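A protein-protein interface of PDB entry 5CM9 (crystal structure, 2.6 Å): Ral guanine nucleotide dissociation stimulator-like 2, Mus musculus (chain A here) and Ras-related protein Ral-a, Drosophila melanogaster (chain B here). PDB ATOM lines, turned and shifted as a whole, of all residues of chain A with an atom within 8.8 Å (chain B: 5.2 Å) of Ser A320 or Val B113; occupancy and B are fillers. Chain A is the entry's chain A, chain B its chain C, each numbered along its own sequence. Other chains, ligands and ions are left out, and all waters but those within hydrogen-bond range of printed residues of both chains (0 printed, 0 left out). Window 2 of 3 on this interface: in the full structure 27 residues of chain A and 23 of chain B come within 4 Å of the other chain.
Along chain A the printed residues that touch a printed residue of chain B span positions 318 to 463.
Along chain B the printed residues that touch a printed residue of chain A span positions 79 to 113.
The backbone NH (N) of Ser A320 sits at hydrogen-bond distance from the side-chain carboxylate (OD2) of Asp B79 (3.1 Å).
OE2 of Glu A459 is in salt-bridge range of NH1 of Arg B112.
The guanidinium group (NH2) of Arg B83 lies within hydrogen-bond range of the backbone carbonyl oxygen (O) of Gln A318 (2.4 Å).
OG of Ser A319 touches OD2 of Asp B79 (3.6 Å).
C of Ser A319 touches NH2 of Arg B83, 3.7 Å away.
Arg B83 touches Ser A320 (NH2 to N, 3.6 Å).
Arg B112 touches Ser A320.
Ser A320 touches Val B113 (CB to CA, 3.9 Å).
CB of His A323 touches NH2 of Arg B83, 3.6 Å away.
Glu A459 touches Gln B109 (OE2 to CG, 3.3 Å).
His A463 touches Arg B112 (CD2 to CG, 3.7 Å).
Ser A320 touches four residues of chain B.
Val B113 touches just one residue of chain A: Ser A320 (3.9 Å).
Of the printed residues of chain A, Asp B79 touches Ser A319 (3.6 Å) and Ser A320 (3.1 Å).
Of the printed residues of chain A, Gln B109 touches Glu A459 (3.3 Å).
The nearest printed residue of chain B that does not touch Ser A320 is Gln B109 (5.9 Å).
The backbone carbonyl oxygen (O) of His A463 is in hydrogen-bond range of the side-chain sulfur (SG) of Cys A467 (3.7 Å).
The side-chain carboxylate of Asp B79 is in salt-bridge range of the guanidinium group of Arg B83.
O of Glu A459 sits at hydrogen-bond distance from OG of Ser A462, at 3.0 Å.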
ATOM      1  N   VAL A 261       5.300   5.425  13.726  1.00  0.00           N
ATOM      2  CA  VAL A 261       6.638   5.774  14.203  1.00  0.00           C
ATOM      3  C   VAL A 261       7.535   6.240  13.056  1.00  0.00           C
ATOM      4  O   VAL A 261       8.227   7.250  13.172  1.00  0.00           O
ATOM      5  CB  VAL A 261       7.296   4.591  14.968  1.00  0.00           C
ATOM      6  CG1 VAL A 261       8.774   4.852  15.212  1.00  0.00           C
ATOM      7  CG2 VAL A 261       6.578   4.347  16.290  1.00  0.00           C
ATOM      8  N   LEU A 265       8.688  10.274  12.259  1.00  0.00           N
ATOM      9  CA  LEU A 265      10.128  10.498  12.122  1.00  0.00           C
ATOM     10  C   LEU A 265      10.550  10.812  10.682  1.00  0.00           C
ATOM     11  O   LEU A 265      11.672  11.273  10.443  1.00  0.00           O
ATOM     12  CB  LEU A 265      10.919   9.309  12.668  1.00  0.00           C
ATOM     13  CG  LEU A 265      10.839   9.079  14.183  1.00  0.00           C
ATOM     14  CD1 LEU A 265      11.495   7.761  14.569  1.00  0.00           C
ATOM     15  CD2 LEU A 265      11.456  10.232  14.958  1.00  0.00           C
ATOM     16  N   VAL A 314      -2.039   4.941  19.190  1.00  0.00           N
ATOM     17  CA  VAL A 314      -1.901   5.657  20.456  1.00  0.00           C
ATOM     18  C   VAL A 314      -0.623   5.248  21.177  1.00  0.00           C
ATOM     19  O   VAL A 314       0.176   6.101  21.572  1.00  0.00           O
ATOM     20  CB  VAL A 314      -3.159   5.457  21.354  1.00  0.00           C
ATOM     21  CG1 VAL A 314      -2.868   5.749  22.823  1.00  0.00           C
ATOM     22  CG2 VAL A 314      -4.299   6.324  20.854  1.00  0.00           C
ATOM     23  N   SER A 315      -0.419   3.943  21.322  1.00  0.00           N
ATOM     24  CA  SER A 315       0.790   3.442  21.957  1.00  0.00           C
ATOM     25  C   SER A 315       2.026   3.825  21.145  1.00  0.00           C
ATOM     26  O   SER A 315       3.076   4.111  21.714  1.00  0.00           O
ATOM     27  CB  SER A 315       0.711   1.933  22.183  1.00  0.00           C
ATOM     28  OG  SER A 315       0.527   1.249  20.960  1.00  0.00           O
ATOM     29  N   ALA A 316       1.883   3.845  19.821  1.00  0.00           N
ATOM     30  CA  ALA A 316       2.939   4.324  18.924  1.00  0.00           C
ATOM     31  C   ALA A 316       3.247   5.811  19.112  1.00  0.00           C
ATOM     32  O   ALA A 316       4.399   6.216  19.039  1.00  0.00           O
ATOM     33  CB  ALA A 316       2.585   4.040  17.478  1.00  0.00           C
ATOM     34  N   LEU A 317       2.224   6.621  19.349  1.00  0.00           N
ATOM     35  CA  LEU A 317       2.448   8.035  19.637  1.00  0.00           C
ATOM     36  C   LEU A 317       3.044   8.228  21.024  1.00  0.00           C
ATOM     37  O   LEU A 317       3.766   9.193  21.258  1.00  0.00           O
ATOM     38  CB  LEU A 317       1.162   8.856  19.469  1.00  0.00           C
ATOM     39  CG  LEU A 317       0.654   9.041  18.034  1.00  0.00           C
ATOM     40  CD1 LEU A 317      -0.764   9.581  17.996  1.00  0.00           C
ATOM     41  CD2 LEU A 317       1.574   9.929  17.231  1.00  0.00           C
ATOM     42  N   GLN A 318       2.743   7.299  21.933  1.00  0.00           N
ATOM     43  CA  GLN A 318       3.300   7.307  23.290  1.00  0.00           C
ATOM     44  C   GLN A 318       4.645   6.592  23.336  1.00  0.00           C
ATOM     45  O   GLN A 318       5.335   6.624  24.358  1.00  0.00           O
ATOM     46  CB  GLN A 318       2.344   6.645  24.283  1.00  0.00           C
ATOM     47  CG  GLN A 318       1.088   7.446  24.581  1.00  0.00           C
ATOM     48  CD  GLN A 318       0.199   6.776  25.614  1.00  0.00           C
ATOM     49  OE1 GLN A 318      -0.247   7.415  26.567  1.00  0.00           O
ATOM     50  NE2 GLN A 318      -0.055   5.484  25.433  1.00  0.00           N
ATOM     51  N   SER A 319       5.000   5.945  22.229  1.00  0.00           N
ATOM     52  CA  SER A 319       6.277   5.244  22.078  1.00  0.00           C
ATOM     53  C   SER A 319       7.451   6.168  22.401  1.00  0.00           C
ATOM     54  O   SER A 319       7.381   7.376  22.154  1.00  0.00           O
ATOM     55  CB  SER A 319       6.394   4.697  20.656  1.00  0.00           C
ATOM     56  OG  SER A 319       7.622   4.038  20.446  1.00  0.00           O
ATOM     57  N   SER A 320       8.523   5.597  22.946  1.00  0.00           N
ATOM     58  CA  SER A 320       9.630   6.390  23.494  1.00  0.00           C
ATOM     59  C   SER A 320      10.372   7.273  22.475  1.00  0.00           C
ATOM     60  O   SER A 320      10.772   8.382  22.822  1.00  0.00           O
ATOM     61  CB  SER A 320      10.607   5.519  24.304  1.00  0.00           C
ATOM     62  OG  SER A 320      11.489   4.783  23.471  1.00  0.00           O
ATOM     63  N   PRO A 321      10.555   6.799  21.223  1.00  0.00           N
ATOM     64  CA  PRO A 321      11.226   7.679  20.258  1.00  0.00           C
ATOM     65  C   PRO A 321      10.370   8.861  19.778  1.00  0.00           C
ATOM     66  O   PRO A 321      10.889   9.794  19.166  1.00  0.00           O
ATOM     67  CB  PRO A 321      11.542   6.741  19.088  1.00  0.00           C
ATOM     68  CG  PRO A 321      10.554   5.633  19.209  1.00  0.00           C
ATOM     69  CD  PRO A 321      10.350   5.445  20.672  1.00  0.00           C
ATOM     70  N   ILE A 322       9.074   8.825  20.054  1.00  0.00           N
ATOM     71  CA  ILE A 322       8.182   9.881  19.583  1.00  0.00           C
ATOM     72  C   ILE A 322       7.599  10.695  20.738  1.00  0.00           C
ATOM     73  O   ILE A 322       7.179  11.840  20.558  1.00  0.00           O
ATOM     74  CB  ILE A 322       7.110   9.333  18.599  1.00  0.00           C
ATOM     75  CG1 ILE A 322       5.802  10.117  18.697  1.00  0.00           C
ATOM     76  CG2 ILE A 322       6.871   7.852  18.835  1.00  0.00           C
ATOM     77  CD1 ILE A 322       4.926   9.966  17.482  1.00  0.00           C
ATOM     78  N   HIS A 323       7.603  10.100  21.923  1.00  0.00           N
ATOM     79  CA  HIS A 323       7.233  10.794  23.146  1.00  0.00           C
ATOM     80  C   HIS A 323       8.179  11.973  23.411  1.00  0.00           C
ATOM     81  O   HIS A 323       7.745  13.044  23.843  1.00  0.00           O
ATOM     82  CB  HIS A 323       7.238   9.808  24.318  1.00  0.00           C
ATOM     83  CG  HIS A 323       6.947  10.436  25.643  1.00  0.00           C
ATOM     84  ND1 HIS A 323       7.939  10.923  26.467  1.00  0.00           N
ATOM     85  CD2 HIS A 323       5.777  10.655  26.288  1.00  0.00           C
ATOM     86  CE1 HIS A 323       7.391  11.421  27.562  1.00  0.00           C
ATOM     87  NE2 HIS A 323       6.080  11.269  27.479  1.00  0.00           N
ATOM     88  N   ARG A 324       9.465  11.765  23.129  1.00  0.00           N
ATOM     89  CA  ARG A 324      10.510  12.765  23.352  1.00  0.00           C
ATOM     90  C   ARG A 324      10.272  14.073  22.606  1.00  0.00           C
ATOM     91  O   ARG A 324      10.539  15.148  23.140  1.00  0.00           O
ATOM     92  CB  ARG A 324      11.869  12.230  22.901  1.00  0.00           C
ATOM     93  CG  ARG A 324      12.404  11.026  23.650  1.00  0.00           C
ATOM     94  CD  ARG A 324      13.894  10.823  23.351  1.00  0.00           C
ATOM     95  NE  ARG A 324      14.252  11.258  22.000  1.00  0.00           N
ATOM     96  CZ  ARG A 324      14.931  12.368  21.711  1.00  0.00           C
ATOM     97  NH1 ARG A 324      15.354  13.177  22.676  1.00  0.00           N
ATOM     98  NH2 ARG A 324      15.186  12.669  20.446  1.00  0.00           N
ATOM     99  N   LEU A 325       9.788  13.963  21.371  1.00  0.00           N
ATOM    100  CA  LEU A 325       9.739  15.081  20.422  1.00  0.00           C
ATOM    101  C   LEU A 325       8.871  16.258  20.885  1.00  0.00           C
ATOM    102  O   LEU A 325       7.813  16.523  20.313  1.00  0.00           O
ATOM    103  CB  LEU A 325       9.294  14.578  19.038  1.00  0.00           C
ATOM    104  CG  LEU A 325       9.991  13.349  18.432  1.00  0.00           C
ATOM    105  CD1 LEU A 325       9.253  12.871  17.203  1.00  0.00           C
ATOM    106  CD2 LEU A 325      11.446  13.623  18.093  1.00  0.00           C
ATOM    107  N   ARG A 326       9.342  16.967  21.911  1.00  0.00           N
ATOM    108  CA  ARG A 326       8.571  18.030  22.568  1.00  0.00           C
ATOM    109  C   ARG A 326       8.314  19.233  21.664  1.00  0.00           C
ATOM    110  O   ARG A 326       7.206  19.767  21.653  1.00  0.00           O
ATOM    111  CB  ARG A 326       9.244  18.480  23.872  1.00  0.00           C
ATOM    112  CG  ARG A 326       9.156  17.483  25.037  1.00  0.00           C
ATOM    113  CD  ARG A 326       7.785  17.483  25.739  1.00  0.00           C
ATOM    114  NE  ARG A 326       6.864  16.486  25.185  1.00  0.00           N
ATOM    115  CZ  ARG A 326       5.684  16.162  25.715  1.00  0.00           C
ATOM    116  NH1 ARG A 326       5.261  16.748  26.830  1.00  0.00           N
ATOM    117  NH2 ARG A 326       4.923  15.241  25.131  1.00  0.00           N
ATOM    118  N   TRP A 329       5.619  18.226  19.482  1.00  0.00           N
ATOM    119  CA  TRP A 329       4.414  18.097  20.301  1.00  0.00           C
ATOM    120  C   TRP A 329       3.887  19.463  20.730  1.00  0.00           C
ATOM    121  O   TRP A 329       2.682  19.634  20.947  1.00  0.00           O
ATOM    122  CB  TRP A 329       4.654  17.197  21.517  1.00  0.00           C
ATOM    123  CG  TRP A 329       4.497  15.734  21.204  1.00  0.00           C
ATOM    124  CD1 TRP A 329       5.493  14.805  21.087  1.00  0.00           C
ATOM    125  CD2 TRP A 329       3.271  15.038  20.950  1.00  0.00           C
ATOM    126  NE1 TRP A 329       4.963  13.577  20.779  1.00  0.00           N
ATOM    127  CE2 TRP A 329       3.602  13.690  20.689  1.00  0.00           C
ATOM    128  CE3 TRP A 329       1.923  15.423  20.920  1.00  0.00           C
ATOM    129  CZ2 TRP A 329       2.637  12.724  20.400  1.00  0.00           C
ATOM    130  CZ3 TRP A 329       0.962  14.460  20.633  1.00  0.00           C
ATOM    131  CH2 TRP A 329       1.327  13.125  20.375  1.00  0.00           C
ATOM    132  N   GLU A 459      13.167  -0.864  16.217  1.00  0.00           N
ATOM    133  CA  GLU A 459      13.233  -0.117  17.470  1.00  0.00           C
ATOM    134  C   GLU A 459      14.578   0.597  17.629  1.00  0.00           C
ATOM    135  O   GLU A 459      14.639   1.715  18.152  1.00  0.00           O
ATOM    136  CB  GLU A 459      12.978  -1.054  18.649  1.00  0.00           C
ATOM    137  CG  GLU A 459      12.704  -0.355  19.974  1.00  0.00           C
ATOM    138  CD  GLU A 459      12.260  -1.317  21.071  1.00  0.00           C
ATOM    139  OE1 GLU A 459      11.981  -2.499  20.763  1.00  0.00           O
ATOM    140  OE2 GLU A 459      12.186  -0.886  22.245  1.00  0.00           O
ATOM    141  N   SER A 462      14.599   3.583  15.063  1.00  0.00           N
ATOM    142  CA  SER A 462      13.722   4.678  15.464  1.00  0.00           C
ATOM    143  C   SER A 462      14.320   5.534  16.584  1.00  0.00           C
ATOM    144  O   SER A 462      14.129   6.750  16.603  1.00  0.00           O
ATOM    145  CB  SER A 462      12.339   4.150  15.850  1.00  0.00           C
ATOM    146  OG  SER A 462      12.417   3.175  16.872  1.00  0.00           O
ATOM    147  N   HIS A 463      15.056   4.896  17.493  1.00  0.00           N
ATOM    148  CA  HIS A 463      15.710   5.579  18.614  1.00  0.00           C
ATOM    149  C   HIS A 463      16.893   6.439  18.153  1.00  0.00           C
ATOM    150  O   HIS A 463      17.177   7.484  18.740  1.00  0.00           O
ATOM    151  CB  HIS A 463      16.167   4.549  19.652  1.00  0.00           C
ATOM    152  CG  HIS A 463      16.605   5.143  20.957  1.00  0.00           C
ATOM    153  ND1 HIS A 463      17.912   5.501  21.214  1.00  0.00           N
ATOM    154  CD2 HIS A 463      15.911   5.420  22.089  1.00  0.00           C
ATOM    155  CE1 HIS A 463      18.002   5.985  22.440  1.00  0.00           C
ATOM    156  NE2 HIS A 463      16.801   5.947  22.992  1.00  0.00           N
ATOM    157  N   SER A 466      15.294   9.536  16.102  1.00  0.00           N
ATOM    158  CA  SER A 466      14.685  10.463  17.055  1.00  0.00           C
ATOM    159  C   SER A 466      15.713  11.412  17.675  1.00  0.00           C
ATOM    160  O   SER A 466      15.440  12.604  17.848  1.00  0.00           O
ATOM    161  CB  SER A 466      13.950   9.695  18.155  1.00  0.00           C
ATOM    162  OG  SER A 466      13.365  10.580  19.091  1.00  0.00           O
ATOM    163  N   CYS A 467      16.884  10.871  18.012  1.00  0.00           N
ATOM    164  CA  CYS A 467      17.979  11.659  18.580  1.00  0.00           C
ATOM    165  C   CYS A 467      18.596  12.617  17.557  1.00  0.00           C
ATOM    166  O   CYS A 467      18.941  13.749  17.894  1.00  0.00           O
ATOM    167  CB  CYS A 467      19.049  10.745  19.196  1.00  0.00           C
ATOM    168  SG  CYS A 467      18.632  10.111  20.855  1.00  0.00           S
ATOM    169  N   ASP B  79       6.425  -0.594  25.722  1.00  0.00           N
ATOM    170  CA  ASP B  79       6.992   0.750  25.831  1.00  0.00           C
ATOM    171  C   ASP B  79       6.176   1.619  26.788  1.00  0.00           C
ATOM    172  O   ASP B  79       6.735   2.385  27.575  1.00  0.00           O
ATOM    173  CB  ASP B  79       7.045   1.400  24.444  1.00  0.00           C
ATOM    174  CG  ASP B  79       7.990   2.586  24.377  1.00  0.00           C
ATOM    175  OD1 ASP B  79       7.865   3.513  25.205  1.00  0.00           O
ATOM    176  OD2 ASP B  79       8.852   2.598  23.474  1.00  0.00           O
ATOM    177  N   PHE B  82       6.666   0.409  30.430  1.00  0.00           N
ATOM    178  CA  PHE B  82       7.975   0.780  30.978  1.00  0.00           C
ATOM    179  C   PHE B  82       8.093   2.262  31.358  1.00  0.00           C
ATOM    180  O   PHE B  82       8.964   2.631  32.145  1.00  0.00           O
ATOM    181  CB  PHE B  82       9.121   0.376  30.036  1.00  0.00           C
ATOM    182  CG  PHE B  82       9.126  -1.083  29.645  1.00  0.00           C
ATOM    183  CD1 PHE B  82       8.459  -2.041  30.406  1.00  0.00           C
ATOM    184  CD2 PHE B  82       9.827  -1.501  28.521  1.00  0.00           C
ATOM    185  CE1 PHE B  82       8.468  -3.381  30.037  1.00  0.00           C
ATOM    186  CE2 PHE B  82       9.849  -2.843  28.149  1.00  0.00           C
ATOM    187  CZ  PHE B  82       9.170  -3.784  28.910  1.00  0.00           C
ATOM    188  N   ARG B  83       7.225   3.102  30.800  1.00  0.00           N
ATOM    189  CA  ARG B  83       7.197   4.520  31.159  1.00  0.00           C
ATOM    190  C   ARG B  83       6.745   4.713  32.607  1.00  0.00           C
ATOM    191  O   ARG B  83       7.384   5.437  33.374  1.00  0.00           O
ATOM    192  CB  ARG B  83       6.275   5.300  30.215  1.00  0.00           C
ATOM    193  CG  ARG B  83       6.161   6.803  30.522  1.00  0.00           C
ATOM    194  CD  ARG B  83       6.964   7.669  29.554  1.00  0.00           C
ATOM    195  NE  ARG B  83       6.624   7.375  28.163  1.00  0.00           N
ATOM    196  CZ  ARG B  83       7.471   6.861  27.276  1.00  0.00           C
ATOM    197  NH1 ARG B  83       8.728   6.607  27.614  1.00  0.00           N
ATOM    198  NH2 ARG B  83       7.063   6.616  26.041  1.00  0.00           N
ATOM    199  N   GLN B 109      15.393  -2.427  25.808  1.00  0.00           N
ATOM    200  CA  GLN B 109      14.107  -1.732  25.685  1.00  0.00           C
ATOM    201  C   GLN B 109      13.832  -0.833  26.888  1.00  0.00           C
ATOM    202  O   GLN B 109      13.379   0.302  26.731  1.00  0.00           O
ATOM    203  CB  GLN B 109      12.961  -2.738  25.512  1.00  0.00           C
ATOM    204  CG  GLN B 109      12.953  -3.484  24.175  1.00  0.00           C
ATOM    205  CD  GLN B 109      12.277  -4.851  24.254  1.00  0.00           C
ATOM    206  OE1 GLN B 109      11.639  -5.192  25.253  1.00  0.00           O
ATOM    207  NE2 GLN B 109      12.425  -5.643  23.194  1.00  0.00           N
ATOM    208  N   ILE B 110      14.121  -1.348  28.083  1.00  0.00           N
ATOM    209  CA  ILE B 110      13.923  -0.607  29.330  1.00  0.00           C
ATOM    210  C   ILE B 110      14.818   0.634  29.387  1.00  0.00           C
ATOM    211  O   ILE B 110      14.377   1.703  29.812  1.00  0.00           O
ATOM    212  CB  ILE B 110      14.126  -1.515  30.578  1.00  0.00           C
ATOM    213  CG1 ILE B 110      13.020  -2.573  30.647  1.00  0.00           C
ATOM    214  CG2 ILE B 110      14.136  -0.691  31.863  1.00  0.00           C
ATOM    215  CD1 ILE B 110      13.357  -3.783  31.501  1.00  0.00           C
ATOM    216  N   LEU B 111      16.063   0.491  28.940  1.00  0.00           N
ATOM    217  CA  LEU B 111      16.996   1.616  28.894  1.00  0.00           C
ATOM    218  C   LEU B 111      16.588   2.676  27.866  1.00  0.00           C
ATOM    219  O   LEU B 111      16.831   3.866  28.074  1.00  0.00           O
ATOM    220  CB  LEU B 111      18.429   1.133  28.631  1.00  0.00           C
ATOM    221  CG  LEU B 111      19.174   0.340  29.718  1.00  0.00           C
ATOM    222  CD1 LEU B 111      20.474  -0.234  29.162  1.00  0.00           C
ATOM    223  CD2 LEU B 111      19.452   1.178  30.965  1.00  0.00           C
ATOM    224  N   ARG B 112      15.970   2.241  26.767  1.00  0.00           N
ATOM    225  CA  ARG B 112      15.451   3.155  25.742  1.00  0.00           C
ATOM    226  C   ARG B 112      14.329   4.032  26.288  1.00  0.00           C
ATOM    227  O   ARG B 112      14.328   5.249  26.087  1.00  0.00           O
ATOM    228  CB  ARG B 112      14.946   2.380  24.522  1.00  0.00           C
ATOM    229  CG  ARG B 112      16.015   2.021  23.508  1.00  0.00           C
ATOM    230  CD  ARG B 112      15.503   0.981  22.524  1.00  0.00           C
ATOM    231  NE  ARG B 112      16.577   0.453  21.684  1.00  0.00           N
ATOM    232  CZ  ARG B 112      16.580  -0.762  21.140  1.00  0.00           C
ATOM    233  NH1 ARG B 112      15.572  -1.599  21.345  1.00  0.00           N
ATOM    234  NH2 ARG B 112      17.606  -1.146  20.393  1.00  0.00           N
ATOM    235  N   VAL B 113      13.382   3.399  26.979  1.00  0.00           N
ATOM    236  CA  VAL B 113      12.235   4.087  27.568  1.00  0.00           C
ATOM    237  C   VAL B 113      12.676   4.933  28.760  1.00  0.00           C
ATOM    238  O   VAL B 113      12.468   6.146  28.782  1.00  0.00           O
ATOM    239  CB  VAL B 113      11.137   3.084  28.003  1.00  0.00           C
ATOM    240  CG1 VAL B 113       9.971   3.809  28.645  1.00  0.00           C
ATOM    241  CG2 VAL B 113      10.659   2.260  26.815  1.00  0.00           C
ATOM    242  N   LYS B 114      13.285   4.279  29.744  1.00  0.00           N
ATOM    243  CA  LYS B 114      13.844   4.953  30.905  1.00  0.00           C
ATOM    244  C   LYS B 114      15.326   5.188  30.650  1.00  0.00           C
ATOM    245  O   LYS B 114      16.149   4.300  30.883  1.00  0.00           O
ATOM    246  CB  LYS B 114      13.651   4.096  32.160  1.00  0.00           C
ATOM    247  CG  LYS B 114      12.218   4.003  32.674  1.00  0.00           C
ATOM    248  CD  LYS B 114      11.905   5.112  33.668  1.00  0.00           C
ATOM    249  CE  LYS B 114      10.603   4.841  34.404  1.00  0.00           C
ATOM    250  NZ  LYS B 114      10.414   5.769  35.552  1.00  0.00           N
ATOM    251  N   ASN B 115      15.667   6.378  30.159  1.00  0.00           N
ATOM    252  CA  ASN B 115      17.060   6.694  29.825  1.00  0.00           C
ATOM    253  C   ASN B 115      17.927   6.958  31.062  1.00  0.00           C
ATOM    254  O   ASN B 115      18.346   8.090  31.327  1.00  0.00           O
ATOM    255  CB  ASN B 115      17.145   7.840  28.801  1.00  0.00           C
ATOM    256  CG  ASN B 115      16.346   9.072  29.214  1.00  0.00           C
ATOM    257  OD1 ASN B 115      15.686   9.089  30.258  1.00  0.00           O
ATOM    258  ND2 ASN B 115      16.405  10.113  28.388  1.00  0.00           N
